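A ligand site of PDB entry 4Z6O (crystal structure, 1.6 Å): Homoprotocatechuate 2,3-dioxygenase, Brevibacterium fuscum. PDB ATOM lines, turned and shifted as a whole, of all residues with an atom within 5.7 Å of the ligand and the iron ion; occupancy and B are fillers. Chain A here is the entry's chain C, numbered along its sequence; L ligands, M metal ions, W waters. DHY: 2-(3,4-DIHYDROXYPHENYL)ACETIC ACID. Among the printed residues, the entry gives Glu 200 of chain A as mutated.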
ATOM      1  N   HIS A 155      -5.815  33.379   4.856  1.00  0.00           N
ATOM      2  CA  HIS A 155      -5.474  34.333   3.804  1.00  0.00           C
ATOM      3  C   HIS A 155      -6.671  34.870   3.081  1.00  0.00           C
ATOM      4  O   HIS A 155      -7.785  34.377   3.241  1.00  0.00           O
ATOM      5  CB  HIS A 155      -4.520  33.679   2.788  1.00  0.00           C
ATOM      6  CG  HIS A 155      -5.090  32.526   2.035  1.00  0.00           C
ATOM      7  ND1 HIS A 155      -4.924  31.212   2.413  1.00  0.00           N
ATOM      8  CD2 HIS A 155      -5.814  32.480   0.894  1.00  0.00           C
ATOM      9  CE1 HIS A 155      -5.489  30.418   1.531  1.00  0.00           C
ATOM     10  NE2 HIS A 155      -6.063  31.164   0.610  1.00  0.00           N
ATOM     11  N   ASN A 157      -7.711  36.049  -1.151  1.00  0.00           N
ATOM     12  CA  ASN A 157      -7.312  35.912  -2.544  1.00  0.00           C
ATOM     13  C   ASN A 157      -8.120  36.935  -3.342  1.00  0.00           C
ATOM     14  O   ASN A 157      -9.331  37.005  -3.218  1.00  0.00           O
ATOM     15  CB  ASN A 157      -7.492  34.479  -3.045  1.00  0.00           C
ATOM     16  CG  ASN A 157      -6.952  34.265  -4.436  1.00  0.00           C
ATOM     17  OD1 ASN A 157      -7.317  34.967  -5.356  1.00  0.00           O
ATOM     18  ND2 ASN A 157      -6.056  33.323  -4.588  1.00  0.00           N
ATOM     19  N   ILE A 181       2.294  31.113 -11.029  1.00  0.00           N
ATOM     20  CA  ILE A 181       1.958  30.358 -12.230  1.00  0.00           C
ATOM     21  C   ILE A 181       2.210  31.252 -13.439  1.00  0.00           C
ATOM     22  O   ILE A 181       1.689  32.382 -13.483  1.00  0.00           O
ATOM     23  CB  ILE A 181       0.470  29.934 -12.233  1.00  0.00           C
ATOM     24  CG1 ILE A 181       0.169  28.975 -11.088  1.00  0.00           C
ATOM     25  CG2 ILE A 181       0.116  29.327 -13.575  1.00  0.00           C
ATOM     26  CD1 ILE A 181      -1.298  28.642 -10.858  1.00  0.00           C
ATOM     27  N   TRP A 192       1.241  34.137  -5.164  1.00  0.00           N
ATOM     28  CA  TRP A 192       0.909  34.005  -3.755  1.00  0.00           C
ATOM     29  C   TRP A 192       1.984  34.684  -2.935  1.00  0.00           C
ATOM     30  O   TRP A 192       3.132  34.589  -3.267  1.00  0.00           O
ATOM     31  CB  TRP A 192       0.903  32.505  -3.404  1.00  0.00           C
ATOM     32  CG  TRP A 192      -0.318  31.767  -3.913  1.00  0.00           C
ATOM     33  CD1 TRP A 192      -1.353  31.341  -3.140  1.00  0.00           C
ATOM     34  CD2 TRP A 192      -0.592  31.310  -5.241  1.00  0.00           C
ATOM     35  NE1 TRP A 192      -2.309  30.702  -3.932  1.00  0.00           N
ATOM     36  CE2 TRP A 192      -1.864  30.666  -5.221  1.00  0.00           C
ATOM     37  CE3 TRP A 192       0.082  31.402  -6.469  1.00  0.00           C
ATOM     38  CZ2 TRP A 192      -2.431  30.096  -6.353  1.00  0.00           C
ATOM     39  CZ3 TRP A 192      -0.503  30.841  -7.580  1.00  0.00           C
ATOM     40  CH2 TRP A 192      -1.741  30.217  -7.530  1.00  0.00           C
ATOM     41  N   GLU A 200       0.861  32.139   2.122  1.00  0.00           N
ATOM     42  CA  GLU A 200       0.114  33.312   1.722  1.00  0.00           C
ATOM     43  C   GLU A 200      -0.598  33.990   2.889  1.00  0.00           C
ATOM     44  O   GLU A 200      -1.132  33.335   3.775  1.00  0.00           O
ATOM     45  CB  GLU A 200      -0.935  32.919   0.656  1.00  0.00           C
ATOM     46  CG  GLU A 200      -1.648  31.611   1.023  1.00  0.00           C
ATOM     47  CD  GLU A 200      -2.654  31.157  -0.006  1.00  0.00           C
ATOM     48  OE1 GLU A 200      -3.249  32.038  -0.713  1.00  0.00           O
ATOM     49  OE2 GLU A 200      -2.789  29.903  -0.149  1.00  0.00           O
ATOM     50  N   HIS A 214     -11.749  34.811  -2.613  1.00  0.00           N
ATOM     51  CA  HIS A 214     -12.153  34.070  -1.424  1.00  0.00           C
ATOM     52  C   HIS A 214     -11.492  34.574  -0.176  1.00  0.00           C
ATOM     53  O   HIS A 214     -10.481  35.307  -0.224  1.00  0.00           O
ATOM     54  CB  HIS A 214     -11.919  32.554  -1.590  1.00  0.00           C
ATOM     55  CG  HIS A 214     -10.498  32.147  -1.830  1.00  0.00           C
ATOM     56  ND1 HIS A 214      -9.991  31.911  -3.075  1.00  0.00           N
ATOM     57  CD2 HIS A 214      -9.517  31.807  -0.969  1.00  0.00           C
ATOM     58  CE1 HIS A 214      -8.739  31.507  -2.991  1.00  0.00           C
ATOM     59  NE2 HIS A 214      -8.432  31.422  -1.721  1.00  0.00           N
ATOM     60  N   ALA A 216      -9.947  32.509   3.259  1.00  0.00           N
ATOM     61  CA  ALA A 216      -9.586  31.149   3.640  1.00  0.00           C
ATOM     62  C   ALA A 216      -9.356  31.017   5.128  1.00  0.00           C
ATOM     63  O   ALA A 216      -8.654  31.857   5.738  1.00  0.00           O
ATOM     64  CB  ALA A 216      -8.322  30.755   2.945  1.00  0.00           C
ATOM     65  N   ARG A 243     -15.852  23.320  -5.383  1.00  0.00           N
ATOM     66  CA  ARG A 243     -14.634  22.675  -5.918  1.00  0.00           C
ATOM     67  C   ARG A 243     -13.901  21.998  -4.760  1.00  0.00           C
ATOM     68  O   ARG A 243     -13.733  22.583  -3.701  1.00  0.00           O
ATOM     69  CB  ARG A 243     -13.730  23.719  -6.534  1.00  0.00           C
ATOM     70  CG  ARG A 243     -12.352  23.209  -6.956  1.00  0.00           C
ATOM     71  CD  ARG A 243     -11.546  24.192  -7.791  1.00  0.00           C
ATOM     72  NE  ARG A 243     -10.190  23.636  -7.875  1.00  0.00           N
ATOM     73  CZ  ARG A 243      -9.057  24.319  -7.687  1.00  0.00           C
ATOM     74  NH1 ARG A 243      -9.015  25.660  -7.669  1.00  0.00           N
ATOM     75  NH2 ARG A 243      -7.925  23.648  -7.565  1.00  0.00           N
ATOM     76  N   HIS A 248      -3.714  20.834  -3.178  1.00  0.00           N
ATOM     77  CA  HIS A 248      -3.232  21.838  -4.081  1.00  0.00           C
ATOM     78  C   HIS A 248      -1.835  21.430  -4.556  1.00  0.00           C
ATOM     79  O   HIS A 248      -1.048  20.786  -3.802  1.00  0.00           O
ATOM     80  CB  HIS A 248      -3.078  23.188  -3.390  1.00  0.00           C
ATOM     81  CG  HIS A 248      -4.309  23.992  -3.197  1.00  0.00           C
ATOM     82  ND1 HIS A 248      -5.194  24.284  -4.210  1.00  0.00           N
ATOM     83  CD2 HIS A 248      -4.759  24.650  -2.093  1.00  0.00           C
ATOM     84  CE1 HIS A 248      -6.150  25.082  -3.729  1.00  0.00           C
ATOM     85  NE2 HIS A 248      -5.886  25.328  -2.448  1.00  0.00           N
ATOM     86  N   GLY A 249      -1.487  21.833  -5.767  1.00  0.00           N
ATOM     87  CA  GLY A 249      -0.100  21.847  -6.218  1.00  0.00           C
ATOM     88  C   GLY A 249       0.606  23.036  -5.602  1.00  0.00           C
ATOM     89  O   GLY A 249       1.333  22.903  -4.632  1.00  0.00           O
ATOM     90  N   VAL A 250       0.315  24.232  -6.118  1.00  0.00           N
ATOM     91  CA  VAL A 250       0.722  25.441  -5.409  1.00  0.00           C
ATOM     92  C   VAL A 250       0.258  25.403  -3.958  1.00  0.00           C
ATOM     93  O   VAL A 250      -0.924  25.209  -3.705  1.00  0.00           O
ATOM     94  CB  VAL A 250       0.091  26.687  -6.055  1.00  0.00           C
ATOM     95  CG1 VAL A 250       0.352  27.939  -5.194  1.00  0.00           C
ATOM     96  CG2 VAL A 250       0.607  26.849  -7.476  1.00  0.00           C
ATOM     97  N   SER A 251       1.182  25.641  -3.026  1.00  0.00           N
ATOM     98  CA  SER A 251       0.977  25.622  -1.566  1.00  0.00           C
ATOM     99  C   SER A 251       1.061  24.255  -0.912  1.00  0.00           C
ATOM    100  O   SER A 251       1.358  24.187   0.277  1.00  0.00           O
ATOM    101  CB  SER A 251      -0.294  26.289  -1.106  1.00  0.00           C
ATOM    102  OG  SER A 251      -1.429  25.421  -1.177  1.00  0.00           O
ATOM    103  N   TYR A 255      -7.433  21.226   0.558  1.00  0.00           N
ATOM    104  CA  TYR A 255      -8.352  22.369   0.388  1.00  0.00           C
ATOM    105  C   TYR A 255      -9.785  21.967   0.039  1.00  0.00           C
ATOM    106  O   TYR A 255     -10.075  20.856  -0.402  1.00  0.00           O
ATOM    107  CB  TYR A 255      -7.867  23.286  -0.732  1.00  0.00           C
ATOM    108  CG  TYR A 255      -8.036  22.726  -2.128  1.00  0.00           C
ATOM    109  CD1 TYR A 255      -7.041  21.927  -2.714  1.00  0.00           C
ATOM    110  CD2 TYR A 255      -9.176  22.954  -2.850  1.00  0.00           C
ATOM    111  CE1 TYR A 255      -7.193  21.405  -3.986  1.00  0.00           C
ATOM    112  CE2 TYR A 255      -9.349  22.439  -4.110  1.00  0.00           C
ATOM    113  CZ  TYR A 255      -8.372  21.667  -4.692  1.00  0.00           C
ATOM    114  OH  TYR A 255      -8.524  21.129  -5.947  1.00  0.00           O
ATOM    115  N   TYR A 257     -13.380  24.454  -1.529  1.00  0.00           N
ATOM    116  CA  TYR A 257     -14.082  25.734  -1.739  1.00  0.00           C
ATOM    117  C   TYR A 257     -15.597  25.561  -1.638  1.00  0.00           C
ATOM    118  O   TYR A 257     -16.164  24.722  -2.329  1.00  0.00           O
ATOM    119  CB  TYR A 257     -13.760  26.290  -3.114  1.00  0.00           C
ATOM    120  CG  TYR A 257     -12.293  26.609  -3.295  1.00  0.00           C
ATOM    121  CD1 TYR A 257     -11.730  27.819  -2.845  1.00  0.00           C
ATOM    122  CD2 TYR A 257     -11.469  25.702  -3.905  1.00  0.00           C
ATOM    123  CE1 TYR A 257     -10.362  28.072  -3.026  1.00  0.00           C
ATOM    124  CE2 TYR A 257     -10.113  25.953  -4.104  1.00  0.00           C
ATOM    125  CZ  TYR A 257      -9.562  27.128  -3.638  1.00  0.00           C
ATOM    126  OH  TYR A 257      -8.227  27.319  -3.908  1.00  0.00           O
ATOM    127  N   GLU A 267     -12.577  29.383   1.325  1.00  0.00           N
ATOM    128  CA  GLU A 267     -11.708  28.229   1.204  1.00  0.00           C
ATOM    129  C   GLU A 267     -11.462  27.679   2.601  1.00  0.00           C
ATOM    130  O   GLU A 267     -11.258  28.428   3.546  1.00  0.00           O
ATOM    131  CB  GLU A 267     -10.356  28.623   0.515  1.00  0.00           C
ATOM    132  CG  GLU A 267      -9.458  27.395   0.309  1.00  0.00           C
ATOM    133  CD  GLU A 267      -8.143  27.676  -0.340  1.00  0.00           C
ATOM    134  OE1 GLU A 267      -7.775  28.856  -0.353  1.00  0.00           O
ATOM    135  OE2 GLU A 267      -7.511  26.734  -0.857  1.00  0.00           O
ATOM    136  N   TYR A 269      -8.589  25.088   4.345  1.00  0.00           N
ATOM    137  CA  TYR A 269      -7.208  24.907   3.938  1.00  0.00           C
ATOM    138  C   TYR A 269      -6.431  24.322   5.128  1.00  0.00           C
ATOM    139  O   TYR A 269      -6.694  24.659   6.298  1.00  0.00           O
ATOM    140  CB  TYR A 269      -6.693  26.320   3.655  1.00  0.00           C
ATOM    141  CG  TYR A 269      -5.323  26.606   3.134  1.00  0.00           C
ATOM    142  CD1 TYR A 269      -5.097  26.722   1.763  1.00  0.00           C
ATOM    143  CD2 TYR A 269      -4.257  26.914   4.001  1.00  0.00           C
ATOM    144  CE1 TYR A 269      -3.853  27.090   1.267  1.00  0.00           C
ATOM    145  CE2 TYR A 269      -2.997  27.251   3.493  1.00  0.00           C
ATOM    146  CZ  TYR A 269      -2.836  27.397   2.122  1.00  0.00           C
ATOM    147  OH  TYR A 269      -1.611  27.775   1.648  1.00  0.00           O
ATOM    148  N   ARG A 292      -0.947  21.669 -11.116  1.00  0.00           N
ATOM    149  CA  ARG A 292      -0.569  22.924 -10.431  1.00  0.00           C
ATOM    150  C   ARG A 292      -1.587  23.435  -9.447  1.00  0.00           C
ATOM    151  O   ARG A 292      -1.255  24.105  -8.494  1.00  0.00           O
ATOM    152  CB  ARG A 292      -0.275  24.013 -11.483  1.00  0.00           C
ATOM    153  CG  ARG A 292      -1.510  24.666 -12.102  1.00  0.00           C
ATOM    154  CD  ARG A 292      -1.309  25.413 -13.408  1.00  0.00           C
ATOM    155  NE  ARG A 292      -2.636  25.918 -13.799  1.00  0.00           N
ATOM    156  CZ  ARG A 292      -3.585  25.179 -14.348  1.00  0.00           C
ATOM    157  NH1 ARG A 292      -3.383  23.906 -14.634  1.00  0.00           N
ATOM    158  NH2 ARG A 292      -4.762  25.729 -14.611  1.00  0.00           N
ATOM    159  N   ARG A 293      -2.856  23.187  -9.743  1.00  0.00           N
ATOM    160  CA  ARG A 293      -3.967  23.684  -8.954  1.00  0.00           C
ATOM    161  C   ARG A 293      -4.461  22.523  -8.097  1.00  0.00           C
ATOM    162  O   ARG A 293      -4.267  22.555  -6.895  1.00  0.00           O
ATOM    163  CB  ARG A 293      -5.055  24.367  -9.786  1.00  0.00           C
ATOM    164  CG  ARG A 293      -4.598  25.769 -10.217  1.00  0.00           C
ATOM    165  CD  ARG A 293      -5.704  26.683 -10.667  1.00  0.00           C
ATOM    166  NE  ARG A 293      -5.227  28.033 -10.995  1.00  0.00           N
ATOM    167  CZ  ARG A 293      -5.077  29.048 -10.131  1.00  0.00           C
ATOM    168  NH1 ARG A 293      -5.250  28.895  -8.842  1.00  0.00           N
ATOM    169  NH2 ARG A 293      -4.656  30.201 -10.589  1.00  0.00           N
ATOM    170  N   ASP A 294      -5.033  21.510  -8.730  1.00  0.00           N
ATOM    171  CA  ASP A 294      -5.318  20.293  -8.022  1.00  0.00           C
ATOM    172  C   ASP A 294      -4.214  19.290  -8.387  1.00  0.00           C
ATOM    173  O   ASP A 294      -4.055  18.900  -9.539  1.00  0.00           O
ATOM    174  CB  ASP A 294      -6.685  19.748  -8.415  1.00  0.00           C
ATOM    175  CG  ASP A 294      -7.081  18.574  -7.560  1.00  0.00           C
ATOM    176  OD1 ASP A 294      -7.584  18.845  -6.417  1.00  0.00           O
ATOM    177  OD2 ASP A 294      -6.867  17.420  -8.004  1.00  0.00           O
ATOM    178  N   VAL A 300     -10.626  22.014 -12.772  1.00  0.00           N
ATOM    179  CA  VAL A 300     -11.053  23.241 -12.098  1.00  0.00           C
ATOM    180  C   VAL A 300     -12.317  23.708 -12.814  1.00  0.00           C
ATOM    181  O   VAL A 300     -12.298  24.059 -13.987  1.00  0.00           O
ATOM    182  CB  VAL A 300      -9.941  24.307 -12.153  1.00  0.00           C
ATOM    183  CG1 VAL A 300     -10.351  25.567 -11.441  1.00  0.00           C
ATOM    184  CG2 VAL A 300      -8.676  23.763 -11.484  1.00  0.00           C
ATOM    185  N   TRP A 304     -14.977  28.757 -10.824  1.00  0.00           N
ATOM    186  CA  TRP A 304     -13.814  29.123  -9.998  1.00  0.00           C
ATOM    187  C   TRP A 304     -12.965  30.229 -10.639  1.00  0.00           C
ATOM    188  O   TRP A 304     -12.459  31.138  -9.964  1.00  0.00           O
ATOM    189  CB  TRP A 304     -12.969  27.873  -9.674  1.00  0.00           C
ATOM    190  CG  TRP A 304     -12.084  28.067  -8.522  1.00  0.00           C
ATOM    191  CD1 TRP A 304     -12.400  27.817  -7.223  1.00  0.00           C
ATOM    192  CD2 TRP A 304     -10.759  28.627  -8.509  1.00  0.00           C
ATOM    193  NE1 TRP A 304     -11.385  28.134  -6.427  1.00  0.00           N
ATOM    194  CE2 TRP A 304     -10.351  28.655  -7.170  1.00  0.00           C
ATOM    195  CE3 TRP A 304      -9.915  29.149  -9.467  1.00  0.00           C
ATOM    196  CZ2 TRP A 304      -9.126  29.144  -6.762  1.00  0.00           C
ATOM    197  CZ3 TRP A 304      -8.695  29.647  -9.072  1.00  0.00           C
ATOM    198  CH2 TRP A 304      -8.313  29.653  -7.732  1.00  0.00           C
HETATM  199  C1  DHY L   1      -4.314  27.400  -5.034  1.00  0.00           C
HETATM  200  C2  DHY L   1      -5.483  28.176  -4.766  1.00  0.00           C
HETATM  201  C3  DHY L   1      -5.696  28.717  -3.487  1.00  0.00           C
HETATM  202  C4  DHY L   1      -4.692  28.539  -2.508  1.00  0.00           C
HETATM  203  C5  DHY L   1      -3.517  27.787  -2.798  1.00  0.00           C
HETATM  204  C6  DHY L   1      -3.354  27.186  -4.055  1.00  0.00           C
HETATM  205  C7  DHY L   1      -4.234  26.732  -6.402  1.00  0.00           C
HETATM  206  C8  DHY L   1      -5.557  26.083  -6.817  1.00  0.00           C
HETATM  207  O1  DHY L   1      -5.778  24.912  -6.574  1.00  0.00           O
HETATM  208  O2  DHY L   1      -6.297  26.702  -7.407  1.00  0.00           O
HETATM  209  O3  DHY L   1      -6.823  29.393  -3.210  1.00  0.00           O
HETATM  210  O4  DHY L   1      -4.927  29.056  -1.303  1.00  0.00           O
HETATM  211 FE    FE M   1      -6.641  30.202  -1.358  1.00  0.00          FE
HETATM  212  O   HOH W   1      -5.215  31.702  -2.477  1.00  0.00           O
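O1 of the ligand sits at hydrogen-bond distance from ND1 of His 248 (2.5 Å). An oxygen (O4) of the ligand lies close to the side-chain carboxylate (OE2) of Glu 200. The side-chain hydroxyl (OH) of Tyr 257 lies close to an oxygen (O3) of the ligand, at 2.6 Å. NH2 of Arg 243 lies within salt-bridge range of O1 of the ligand, at 2.7 Å. The backbone carbonyl oxygen of Arg 293 lies close to an oxygen (O1) of the ligand (2.8 Å). The guanidinium group (NH1) of Arg 293 lies within salt-bridge range of an oxygen (O2) of the ligand (2.8 Å).
Water W1 lies within hydrogen-bond range of OE1 of Glu 200, ND2 of Asn 157 and NE1 of Trp 192.
A ring nitrogen (NE2) of His 248 sits at hydrogen-bond distance from the side-chain carboxylate (OE2) of Glu 267 (2.7 Å). The backbone carbonyl oxygen (O) of His 214 is in hydrogen-bond range of the backbone NH (N) of Asn 157 (3.0 Å). OE1 of Glu 200 sits close to NE2 of His 155 (3.2 Å). NE2 of His 248 sits close to OH of Tyr 257 (3.4 Å). The backbone carbonyl oxygen (O) of Arg 243 is in hydrogen-bond range of the backbone NH (N) of Tyr 257, 2.9 Å away. The side-chain hydroxyl (OH) of Tyr 255 is in hydrogen-bond range of the guanidinium group (NH2) of Arg 243, 3.1 Å away. The backbone carbonyl oxygen (O) of Arg 293 sits at hydrogen-bond distance from the backbone NH (N) of Gly 249, 3.1 Å away. O of Arg 292 sits at hydrogen-bond distance from N of Val 250 (2.9 Å).
Residues that only touch the ligand: Trp 192 (3.4 Å), Val 250 (3.2 Å), Ser 251 (3.5 Å), Tyr 269 (3.4 Å) and Trp 304 (3.6 Å). Hydrophobic or aromatic side chains that line the ligand: His 155, Trp 192, His 214, His 248, Val 250, Tyr 257, Tyr 269 and Trp 304. 13 residues have an atom within 4 Å of the ligand: His 155, Trp 192, Glu 200, His 214, Arg 243, His 248, Val 250, Ser 251, Tyr 257, Glu 267, Tyr 269, Arg 293 and Trp 304.
Glu 200 touches the iron ion (OE1 to FE, 3.9 Å). Within 4 Å of the iron ion: His 155, Glu 200, His 214 and Glu 267.
OE1 of Glu 267 is bound to the iron ion (2.0 Å). The iron ion is bound by O3 of the ligand (2.0 Å). The iron ion is bound by O4 of the ligand, 2.1 Å away. NE2 of His 214 is bound to the iron ion. The iron ion is bound by a ring nitrogen (NE2) of His 155. Water W1 binds the iron ion (2.4 Å).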
